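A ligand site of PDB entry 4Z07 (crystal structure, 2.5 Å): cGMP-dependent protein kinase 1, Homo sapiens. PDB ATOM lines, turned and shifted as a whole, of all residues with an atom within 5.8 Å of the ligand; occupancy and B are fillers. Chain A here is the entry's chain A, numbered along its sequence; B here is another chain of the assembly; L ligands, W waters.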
ATOM      1  N   ASN A  27      34.305  20.667  18.202  1.00  0.00           N
ATOM      2  CA  ASN A  27      33.150  20.469  17.335  1.00  0.00           C
ATOM      3  C   ASN A  27      33.068  21.566  16.276  1.00  0.00           C
ATOM      4  O   ASN A  27      33.073  22.750  16.617  1.00  0.00           O
ATOM      5  CB  ASN A  27      31.878  20.448  18.183  1.00  0.00           C
ATOM      6  CG  ASN A  27      30.626  20.356  17.354  1.00  0.00           C
ATOM      7  OD1 ASN A  27      30.066  21.365  16.924  1.00  0.00           O
ATOM      8  ND2 ASN A  27      30.152  19.131  17.140  1.00  0.00           N
ATOM      9  N   ILE A  57      19.034   9.013  20.260  1.00  0.00           N
ATOM     10  CA  ILE A  57      18.498   9.938  19.279  1.00  0.00           C
ATOM     11  C   ILE A  57      18.003   9.198  18.067  1.00  0.00           C
ATOM     12  O   ILE A  57      18.739   8.401  17.508  1.00  0.00           O
ATOM     13  CB  ILE A  57      19.570  10.956  18.794  1.00  0.00           C
ATOM     14  CG1 ILE A  57      19.845  12.014  19.841  1.00  0.00           C
ATOM     15  CG2 ILE A  57      19.131  11.661  17.533  1.00  0.00           C
ATOM     16  CD1 ILE A  57      20.981  12.947  19.422  1.00  0.00           C
ATOM     17  N   VAL A  76      26.644   6.127  15.010  1.00  0.00           N
ATOM     18  CA  VAL A  76      25.814   7.068  14.249  1.00  0.00           C
ATOM     19  C   VAL A  76      25.447   6.524  12.887  1.00  0.00           C
ATOM     20  O   VAL A  76      26.306   6.208  12.062  1.00  0.00           O
ATOM     21  CB  VAL A  76      26.515   8.405  14.096  1.00  0.00           C
ATOM     22  CG1 VAL A  76      25.620   9.381  13.373  1.00  0.00           C
ATOM     23  CG2 VAL A  76      26.893   8.952  15.486  1.00  0.00           C
ATOM     24  N   LYS A  78      22.542   6.845   9.446  1.00  0.00           N
ATOM     25  CA  LYS A  78      21.531   7.645   8.758  1.00  0.00           C
ATOM     26  C   LYS A  78      20.936   6.795   7.675  1.00  0.00           C
ATOM     27  O   LYS A  78      21.664   6.335   6.783  1.00  0.00           O
ATOM     28  CB  LYS A  78      22.144   8.902   8.162  1.00  0.00           C
ATOM     29  CG  LYS A  78      21.164   9.883   7.574  1.00  0.00           C
ATOM     30  CD  LYS A  78      21.943  10.967   6.849  1.00  0.00           C
ATOM     31  CE  LYS A  78      21.049  12.027   6.238  1.00  0.00           C
ATOM     32  NZ  LYS A  78      20.435  12.891   7.291  1.00  0.00           N
ATOM     33  N   LEU A  83      27.582   5.932   9.768  1.00  0.00           N
ATOM     34  CA  LEU A  83      28.353   7.135   9.504  1.00  0.00           C
ATOM     35  C   LEU A  83      29.661   7.148  10.259  1.00  0.00           C
ATOM     36  O   LEU A  83      30.714   7.432   9.677  1.00  0.00           O
ATOM     37  CB  LEU A  83      27.558   8.378   9.886  1.00  0.00           C
ATOM     38  CG  LEU A  83      26.290   8.604   9.093  1.00  0.00           C
ATOM     39  CD1 LEU A  83      25.770   9.995   9.409  1.00  0.00           C
ATOM     40  CD2 LEU A  83      26.518   8.386   7.595  1.00  0.00           C
ATOM     41  N   CYS A  84      29.600   6.828  11.554  1.00  0.00           N
ATOM     42  CA  CYS A  84      30.784   6.753  12.407  1.00  0.00           C
ATOM     43  C   CYS A  84      30.459   6.198  13.782  1.00  0.00           C
ATOM     44  O   CYS A  84      29.300   5.986  14.122  1.00  0.00           O
ATOM     45  CB  CYS A  84      31.414   8.125  12.570  1.00  0.00           C
ATOM     46  SG  CYS A  84      30.368   9.269  13.479  1.00  0.00           S
ATOM     47  N   MET A  86      31.519   7.230  17.916  1.00  0.00           N
ATOM     48  CA  MET A  86      32.055   8.375  18.637  1.00  0.00           C
ATOM     49  C   MET A  86      32.433   7.997  20.054  1.00  0.00           C
ATOM     50  O   MET A  86      31.716   7.252  20.717  1.00  0.00           O
ATOM     51  CB  MET A  86      31.050   9.533  18.665  1.00  0.00           C
ATOM     52  CG  MET A  86      30.643  10.042  17.298  1.00  0.00           C
ATOM     53  SD  MET A  86      29.746  11.584  17.445  1.00  0.00           S
ATOM     54  CE  MET A  86      28.238  10.962  18.149  1.00  0.00           C
ATOM     55  N   VAL A  91      30.815  16.076  21.081  1.00  0.00           N
ATOM     56  CA  VAL A  91      29.437  16.586  21.061  1.00  0.00           C
ATOM     57  C   VAL A  91      28.596  15.799  20.076  1.00  0.00           C
ATOM     58  O   VAL A  91      29.080  15.443  19.011  1.00  0.00           O
ATOM     59  CB  VAL A  91      29.395  18.073  20.649  1.00  0.00           C
ATOM     60  CG1 VAL A  91      27.949  18.546  20.433  1.00  0.00           C
ATOM     61  CG2 VAL A  91      30.124  18.933  21.671  1.00  0.00           C
ATOM     62  N   PHE A  92      27.358  15.497  20.441  1.00  0.00           N
ATOM     63  CA  PHE A  92      26.385  15.122  19.415  1.00  0.00           C
ATOM     64  C   PHE A  92      25.010  15.647  19.777  1.00  0.00           C
ATOM     65  O   PHE A  92      24.726  15.943  20.939  1.00  0.00           O
ATOM     66  CB  PHE A  92      26.354  13.605  19.188  1.00  0.00           C
ATOM     67  CG  PHE A  92      25.980  12.799  20.406  1.00  0.00           C
ATOM     68  CD1 PHE A  92      24.662  12.448  20.646  1.00  0.00           C
ATOM     69  CD2 PHE A  92      26.951  12.345  21.290  1.00  0.00           C
ATOM     70  CE1 PHE A  92      24.320  11.674  21.742  1.00  0.00           C
ATOM     71  CE2 PHE A  92      26.604  11.570  22.399  1.00  0.00           C
ATOM     72  CZ  PHE A  92      25.291  11.243  22.620  1.00  0.00           C
ATOM     73  N   GLY A  93      24.168  15.798  18.750  1.00  0.00           N
ATOM     74  CA  GLY A  93      22.831  16.309  18.898  1.00  0.00           C
ATOM     75  C   GLY A  93      22.740  17.813  18.811  1.00  0.00           C
ATOM     76  O   GLY A  93      21.719  18.422  19.164  1.00  0.00           O
ATOM     77  N   GLU A  94      23.800  18.444  18.313  1.00  0.00           N
ATOM     78  CA  GLU A  94      23.782  19.887  18.204  1.00  0.00           C
ATOM     79  C   GLU A  94      23.138  20.359  16.887  1.00  0.00           C
ATOM     80  O   GLU A  94      22.629  21.469  16.802  1.00  0.00           O
ATOM     81  CB  GLU A  94      25.211  20.444  18.340  1.00  0.00           C
ATOM     82  CG  GLU A  94      26.020  20.453  17.060  1.00  0.00           C
ATOM     83  CD  GLU A  94      26.492  19.064  16.619  1.00  0.00           C
ATOM     84  OE1 GLU A  94      25.869  18.047  16.998  1.00  0.00           O
ATOM     85  OE2 GLU A  94      27.517  19.007  15.905  1.00  0.00           O
ATOM     86  N   LEU A  95      23.104  19.501  15.863  1.00  0.00           N
ATOM     87  CA  LEU A  95      22.613  19.974  14.568  1.00  0.00           C
ATOM     88  C   LEU A  95      21.130  20.358  14.598  1.00  0.00           C
ATOM     89  O   LEU A  95      20.757  21.430  14.107  1.00  0.00           O
ATOM     90  CB  LEU A  95      22.852  18.921  13.463  1.00  0.00           C
ATOM     91  CG  LEU A  95      24.324  18.595  13.166  1.00  0.00           C
ATOM     92  CD1 LEU A  95      24.429  17.549  12.071  1.00  0.00           C
ATOM     93  CD2 LEU A  95      25.175  19.843  12.853  1.00  0.00           C
ATOM     94  N   ALA A  96      20.297  19.509  15.186  1.00  0.00           N
ATOM     95  CA  ALA A  96      18.854  19.786  15.225  1.00  0.00           C
ATOM     96  C   ALA A  96      18.545  21.083  15.952  1.00  0.00           C
ATOM     97  O   ALA A  96      17.609  21.806  15.585  1.00  0.00           O
ATOM     98  CB  ALA A  96      18.126  18.647  15.882  1.00  0.00           C
ATOM     99  N   ILE A  97      19.361  21.382  16.958  1.00  0.00           N
ATOM    100  CA  ILE A  97      19.148  22.528  17.834  1.00  0.00           C
ATOM    101  C   ILE A  97      19.718  23.823  17.224  1.00  0.00           C
ATOM    102  O   ILE A  97      19.088  24.880  17.294  1.00  0.00           O
ATOM    103  CB  ILE A  97      19.791  22.294  19.212  1.00  0.00           C
ATOM    104  CG1 ILE A  97      19.412  20.922  19.785  1.00  0.00           C
ATOM    105  CG2 ILE A  97      19.408  23.404  20.157  1.00  0.00           C
ATOM    106  CD1 ILE A  97      17.932  20.728  19.994  1.00  0.00           C
ATOM    107  N   CYS A 101      16.059  22.014  12.773  1.00  0.00           N
ATOM    108  CA  CYS A 101      15.571  20.964  11.917  1.00  0.00           C
ATOM    109  C   CYS A 101      15.371  19.746  12.813  1.00  0.00           C
ATOM    110  O   CYS A 101      15.779  19.757  13.992  1.00  0.00           O
ATOM    111  CB  CYS A 101      16.572  20.681  10.800  1.00  0.00           C
ATOM    112  SG  CYS A 101      18.219  20.116  11.363  1.00  0.00           S
ATOM    113  N   THR A 102      14.780  18.688  12.267  1.00  0.00           N
ATOM    114  CA  THR A 102      14.671  17.416  12.975  1.00  0.00           C
ATOM    115  C   THR A 102      16.035  16.720  13.009  1.00  0.00           C
ATOM    116  O   THR A 102      16.952  17.090  12.264  1.00  0.00           O
ATOM    117  CB  THR A 102      13.642  16.475  12.303  1.00  0.00           C
ATOM    118  OG1 THR A 102      14.020  16.249  10.938  1.00  0.00           O
ATOM    119  CG2 THR A 102      12.257  17.073  12.346  1.00  0.00           C
ATOM    120  N   ARG A 103      16.165  15.728  13.888  1.00  0.00           N
ATOM    121  CA  ARG A 103      17.411  14.969  14.001  1.00  0.00           C
ATOM    122  C   ARG A 103      17.825  14.403  12.645  1.00  0.00           C
ATOM    123  O   ARG A 103      17.047  13.746  11.936  1.00  0.00           O
ATOM    124  CB  ARG A 103      17.241  13.837  15.021  1.00  0.00           C
ATOM    125  CG  ARG A 103      16.851  14.323  16.411  1.00  0.00           C
ATOM    126  CD  ARG A 103      18.004  15.109  17.054  1.00  0.00           C
ATOM    127  NE  ARG A 103      17.879  15.238  18.503  1.00  0.00           N
ATOM    128  CZ  ARG A 103      18.673  16.007  19.241  1.00  0.00           C
ATOM    129  NH1 ARG A 103      19.615  16.728  18.649  1.00  0.00           N
ATOM    130  NH2 ARG A 103      18.516  16.087  20.546  1.00  0.00           N
ATOM    131  N   THR A 104      19.076  14.663  12.283  1.00  0.00           N
ATOM    132  CA  THR A 104      19.562  14.347  10.948  1.00  0.00           C
ATOM    133  C   THR A 104      20.180  12.964  10.891  1.00  0.00           C
ATOM    134  O   THR A 104      20.587  12.507   9.828  1.00  0.00           O
ATOM    135  CB  THR A 104      20.630  15.358  10.484  1.00  0.00           C
ATOM    136  OG1 THR A 104      21.793  15.210  11.316  1.00  0.00           O
ATOM    137  CG2 THR A 104      20.100  16.789  10.585  1.00  0.00           C
ATOM    138  N   ALA A 105      20.244  12.290  12.038  1.00  0.00           N
ATOM    139  CA  ALA A 105      20.827  10.957  12.108  1.00  0.00           C
ATOM    140  C   ALA A 105      20.384  10.226  13.373  1.00  0.00           C
ATOM    141  O   ALA A 105      19.784  10.824  14.262  1.00  0.00           O
ATOM    142  CB  ALA A 105      22.342  11.024  12.065  1.00  0.00           C
ATOM    143  N   THR A 106      20.705   8.942  13.450  1.00  0.00           N
ATOM    144  CA  THR A 106      20.358   8.134  14.610  1.00  0.00           C
ATOM    145  C   THR A 106      21.600   7.818  15.448  1.00  0.00           C
ATOM    146  O   THR A 106      22.652   7.444  14.909  1.00  0.00           O
ATOM    147  CB  THR A 106      19.675   6.821  14.187  1.00  0.00           C
ATOM    148  OG1 THR A 106      18.401   7.128  13.610  1.00  0.00           O
ATOM    149  CG2 THR A 106      19.478   5.915  15.377  1.00  0.00           C
ATOM    150  N   VAL A 107      21.470   7.965  16.768  1.00  0.00           N
ATOM    151  CA  VAL A 107      22.568   7.686  17.681  1.00  0.00           C
ATOM    152  C   VAL A 107      22.212   6.601  18.684  1.00  0.00           C
ATOM    153  O   VAL A 107      21.290   6.738  19.481  1.00  0.00           O
ATOM    154  CB  VAL A 107      22.988   8.938  18.454  1.00  0.00           C
ATOM    155  CG1 VAL A 107      24.264   8.646  19.269  1.00  0.00           C
ATOM    156  CG2 VAL A 107      23.210  10.085  17.494  1.00  0.00           C
ATOM    157  N   THR B 136      29.590  17.674   4.483  1.00  0.00           N
ATOM    158  CA  THR B 136      29.136  16.549   5.278  1.00  0.00           C
ATOM    159  C   THR B 136      28.150  15.672   4.498  1.00  0.00           C
ATOM    160  O   THR B 136      28.192  14.454   4.599  1.00  0.00           O
ATOM    161  CB  THR B 136      28.467  17.028   6.590  1.00  0.00           C
ATOM    162  OG1 THR B 136      29.337  17.938   7.267  1.00  0.00           O
ATOM    163  CG2 THR B 136      28.180  15.877   7.502  1.00  0.00           C
ATOM    164  N   GLU B 140      28.347  11.759   3.696  1.00  0.00           N
ATOM    165  CA  GLU B 140      27.291  10.802   3.993  1.00  0.00           C
ATOM    166  C   GLU B 140      26.950   9.986   2.737  1.00  0.00           C
ATOM    167  O   GLU B 140      26.801   8.770   2.810  1.00  0.00           O
ATOM    168  CB  GLU B 140      26.038  11.514   4.528  1.00  0.00           C
ATOM    169  CG  GLU B 140      26.241  12.134   5.923  1.00  0.00           C
ATOM    170  CD  GLU B 140      25.190  13.179   6.284  1.00  0.00           C
ATOM    171  OE1 GLU B 140      25.456  13.957   7.211  1.00  0.00           O
ATOM    172  OE2 GLU B 140      24.124  13.248   5.636  1.00  0.00           O
ATOM    173  N   LYS B 143      29.698   7.436   1.928  1.00  0.00           N
ATOM    174  CA  LYS B 143      29.662   6.327   2.872  1.00  0.00           C
ATOM    175  C   LYS B 143      28.545   5.353   2.513  1.00  0.00           C
ATOM    176  O   LYS B 143      28.603   4.181   2.889  1.00  0.00           O
ATOM    177  CB  LYS B 143      29.485   6.850   4.295  1.00  0.00           C
ATOM    178  CG  LYS B 143      30.743   7.488   4.825  1.00  0.00           C
ATOM    179  CD  LYS B 143      30.471   8.312   6.055  1.00  0.00           C
ATOM    180  CE  LYS B 143      31.739   8.865   6.629  1.00  0.00           C
ATOM    181  NZ  LYS B 143      31.413   9.878   7.644  1.00  0.00           N
HETATM  182  P1  LIG L   1      21.435  15.851  15.337  1.00  0.00           P
HETATM  183  O1  LIG L   1      21.057  15.740  13.738  1.00  0.00           O
HETATM  184  O2  LIG L   1      20.753  16.850  16.143  1.00  0.00           O
HETATM  185  O3  LIG L   1      21.130  14.473  15.924  1.00  0.00           O
HETATM  186  C1  LIG L   1      21.924  13.439  15.114  1.00  0.00           C
HETATM  187  C2  LIG L   1      23.360  13.614  15.450  1.00  0.00           C
HETATM  188  O4  LIG L   1      24.403  12.712  15.041  1.00  0.00           O
HETATM  189  C3  LIG L   1      23.832  14.927  14.893  1.00  0.00           C
HETATM  190  O5  LIG L   1      23.063  16.086  15.371  1.00  0.00           O
HETATM  191  C4  LIG L   1      25.325  14.961  15.129  1.00  0.00           C
HETATM  192  O6  LIG L   1      25.720  15.761  16.191  1.00  0.00           O
HETATM  193  C5  LIG L   1      25.670  13.460  15.148  1.00  0.00           C
HETATM  194  N1  LIG L   1      26.558  13.062  14.026  1.00  0.00           N
HETATM  195  C6  LIG L   1      27.824  12.320  14.125  1.00  0.00           C
HETATM  196  N2  LIG L   1      28.415  12.294  12.788  1.00  0.00           N
HETATM  197  C7  LIG L   1      27.366  12.762  11.859  1.00  0.00           C
HETATM  198  C8  LIG L   1      27.333  12.814  10.360  1.00  0.00           C
HETATM  199  O7  LIG L   1      28.433  12.364   9.644  1.00  0.00           O
HETATM  200  N3  LIG L   1      26.212  13.293   9.700  1.00  0.00           N
HETATM  201  C9  LIG L   1      25.094  13.754  10.440  1.00  0.00           C
HETATM  202  N4  LIG L   1      23.949  14.295   9.745  1.00  0.00           N
HETATM  203  N5  LIG L   1      25.121  13.707  11.946  1.00  0.00           N
HETATM  204  C10 LIG L   1      26.247  13.229  12.592  1.00  0.00           C
HETATM  205  O   HOH W   1      23.285  16.476   7.369  1.00  0.00           O
HETATM  206  O   HOH W   2      28.217  16.745  14.793  1.00  0.00           O
HETATM  207  O   HOH W   3      28.924  14.954  16.427  1.00  0.00           O
HETATM  208  O   HOH W   4      29.950  11.888   7.439  1.00  0.00           O
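Water W4 bridges the side-chain amino group (NZ) of Lys 143 of chain B (2.5 Å) and an oxygen (O7) of the ligand (2.7 Å). Water W2 bridges OE2 of Glu 94 (2.6 Å) and O6 of the ligand (3.0 Å). Water W1 bridges N4 of the ligand (3.3 Å) and OE1 of Glu 140 of chain B (3.3 Å). Water W3 lies within hydrogen-bond range of O of Val 91 (2.6 Å), O6 of the ligand (3.3 Å) and SD of Met 86 (3.6 Å).
Ile 57 touches the ligand (CG2 to O3, 3.8 Å). Val 76 touches the ligand (CG1 to C6, 3.7 Å). CD1 of Leu 83 touches N3 of the ligand, at 3.3 Å. Met 86 touches the ligand (SD to C6, 3.9 Å). CA of Phe 92 touches O6 of the ligand, at 3.4 Å. Ala 105 touches the ligand (O to C1, 3.5 Å). Val 107 touches the ligand (CG2 to O4, 3.8 Å). CG2 of Thr 136 of chain B touches N3 of the ligand, at 3.9 Å. Within 4 Å of the ligand: Ile 57, Val 76, Leu 83, Cys 84, Met 86, Phe 92, Gly 93, Glu 94, Leu 95, Ala 96, Arg 103, Thr 104, Ala 105, Val 107, Thr 136 of chain B and Glu 140 of chain B. Along chain A the residues within 4 Å of the ligand span positions 57 to 107. The nearest printed residue that does not touch the ligand is Lys 143 of chain B (4.4 Å).
The side-chain carboxylate (OE2) of Glu 94 sits at hydrogen-bond distance from the side-chain amide nitrogen (ND2) of Asn 27 (2.9 Å). The backbone carbonyl oxygen of Thr 104 is in hydrogen-bond range of the side-chain amino group of Lys 78, at 2.6 Å. NH1 of Arg 103 lies within hydrogen-bond range of O of Gly 93, 2.7 Å away. The backbone carbonyl oxygen of Ala 96 is in hydrogen-bond range of the backbone NH of Cys 101, at 3.2 Å. The backbone NH of Leu 83 sits at hydrogen-bond distance from the backbone carbonyl oxygen of Val 76 (2.6 Å). The side-chain amino group (NZ) of Lys 143 of chain B is in hydrogen-bond range of the backbone carbonyl oxygen (O) of Leu 83. O of Cys 84 is in hydrogen-bond range of N of Val 76 (2.8 Å). The backbone carbonyl oxygen (O) of Ile 57 is in hydrogen-bond range of the backbone NH (N) of Val 107 (2.9 Å).
The side-chain carboxylate (OE1) of Glu 94 lies within hydrogen-bond range of an oxygen (O6) of the ligand, at 2.4 Å. O1 of the ligand lies within hydrogen-bond range of N of Thr 104. An oxygen (O1) of the ligand lies within hydrogen-bond range of the side-chain hydroxyl (OG1) of Thr 104, at 2.6 Å. N3 of the ligand sits at hydrogen-bond distance from OE1 of Glu 140 of chain B. The guanidinium group (NH1) of Arg 103 is in salt-bridge range of an oxygen (O2) of the ligand (2.8 Å). N of Ala 96 sits at hydrogen-bond distance from O2 of the ligand, 2.9 Å away. N of Gly 93 lies within hydrogen-bond range of O6 of the ligand, 3.0 Å away. The backbone NH (N) of Leu 95 lies close to an oxygen (O5) of the ligand. The side-chain sulfur (SG) of Cys 84 is in hydrogen-bond range of a nitrogen (N2) of the ligand, 3.7 Å away.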
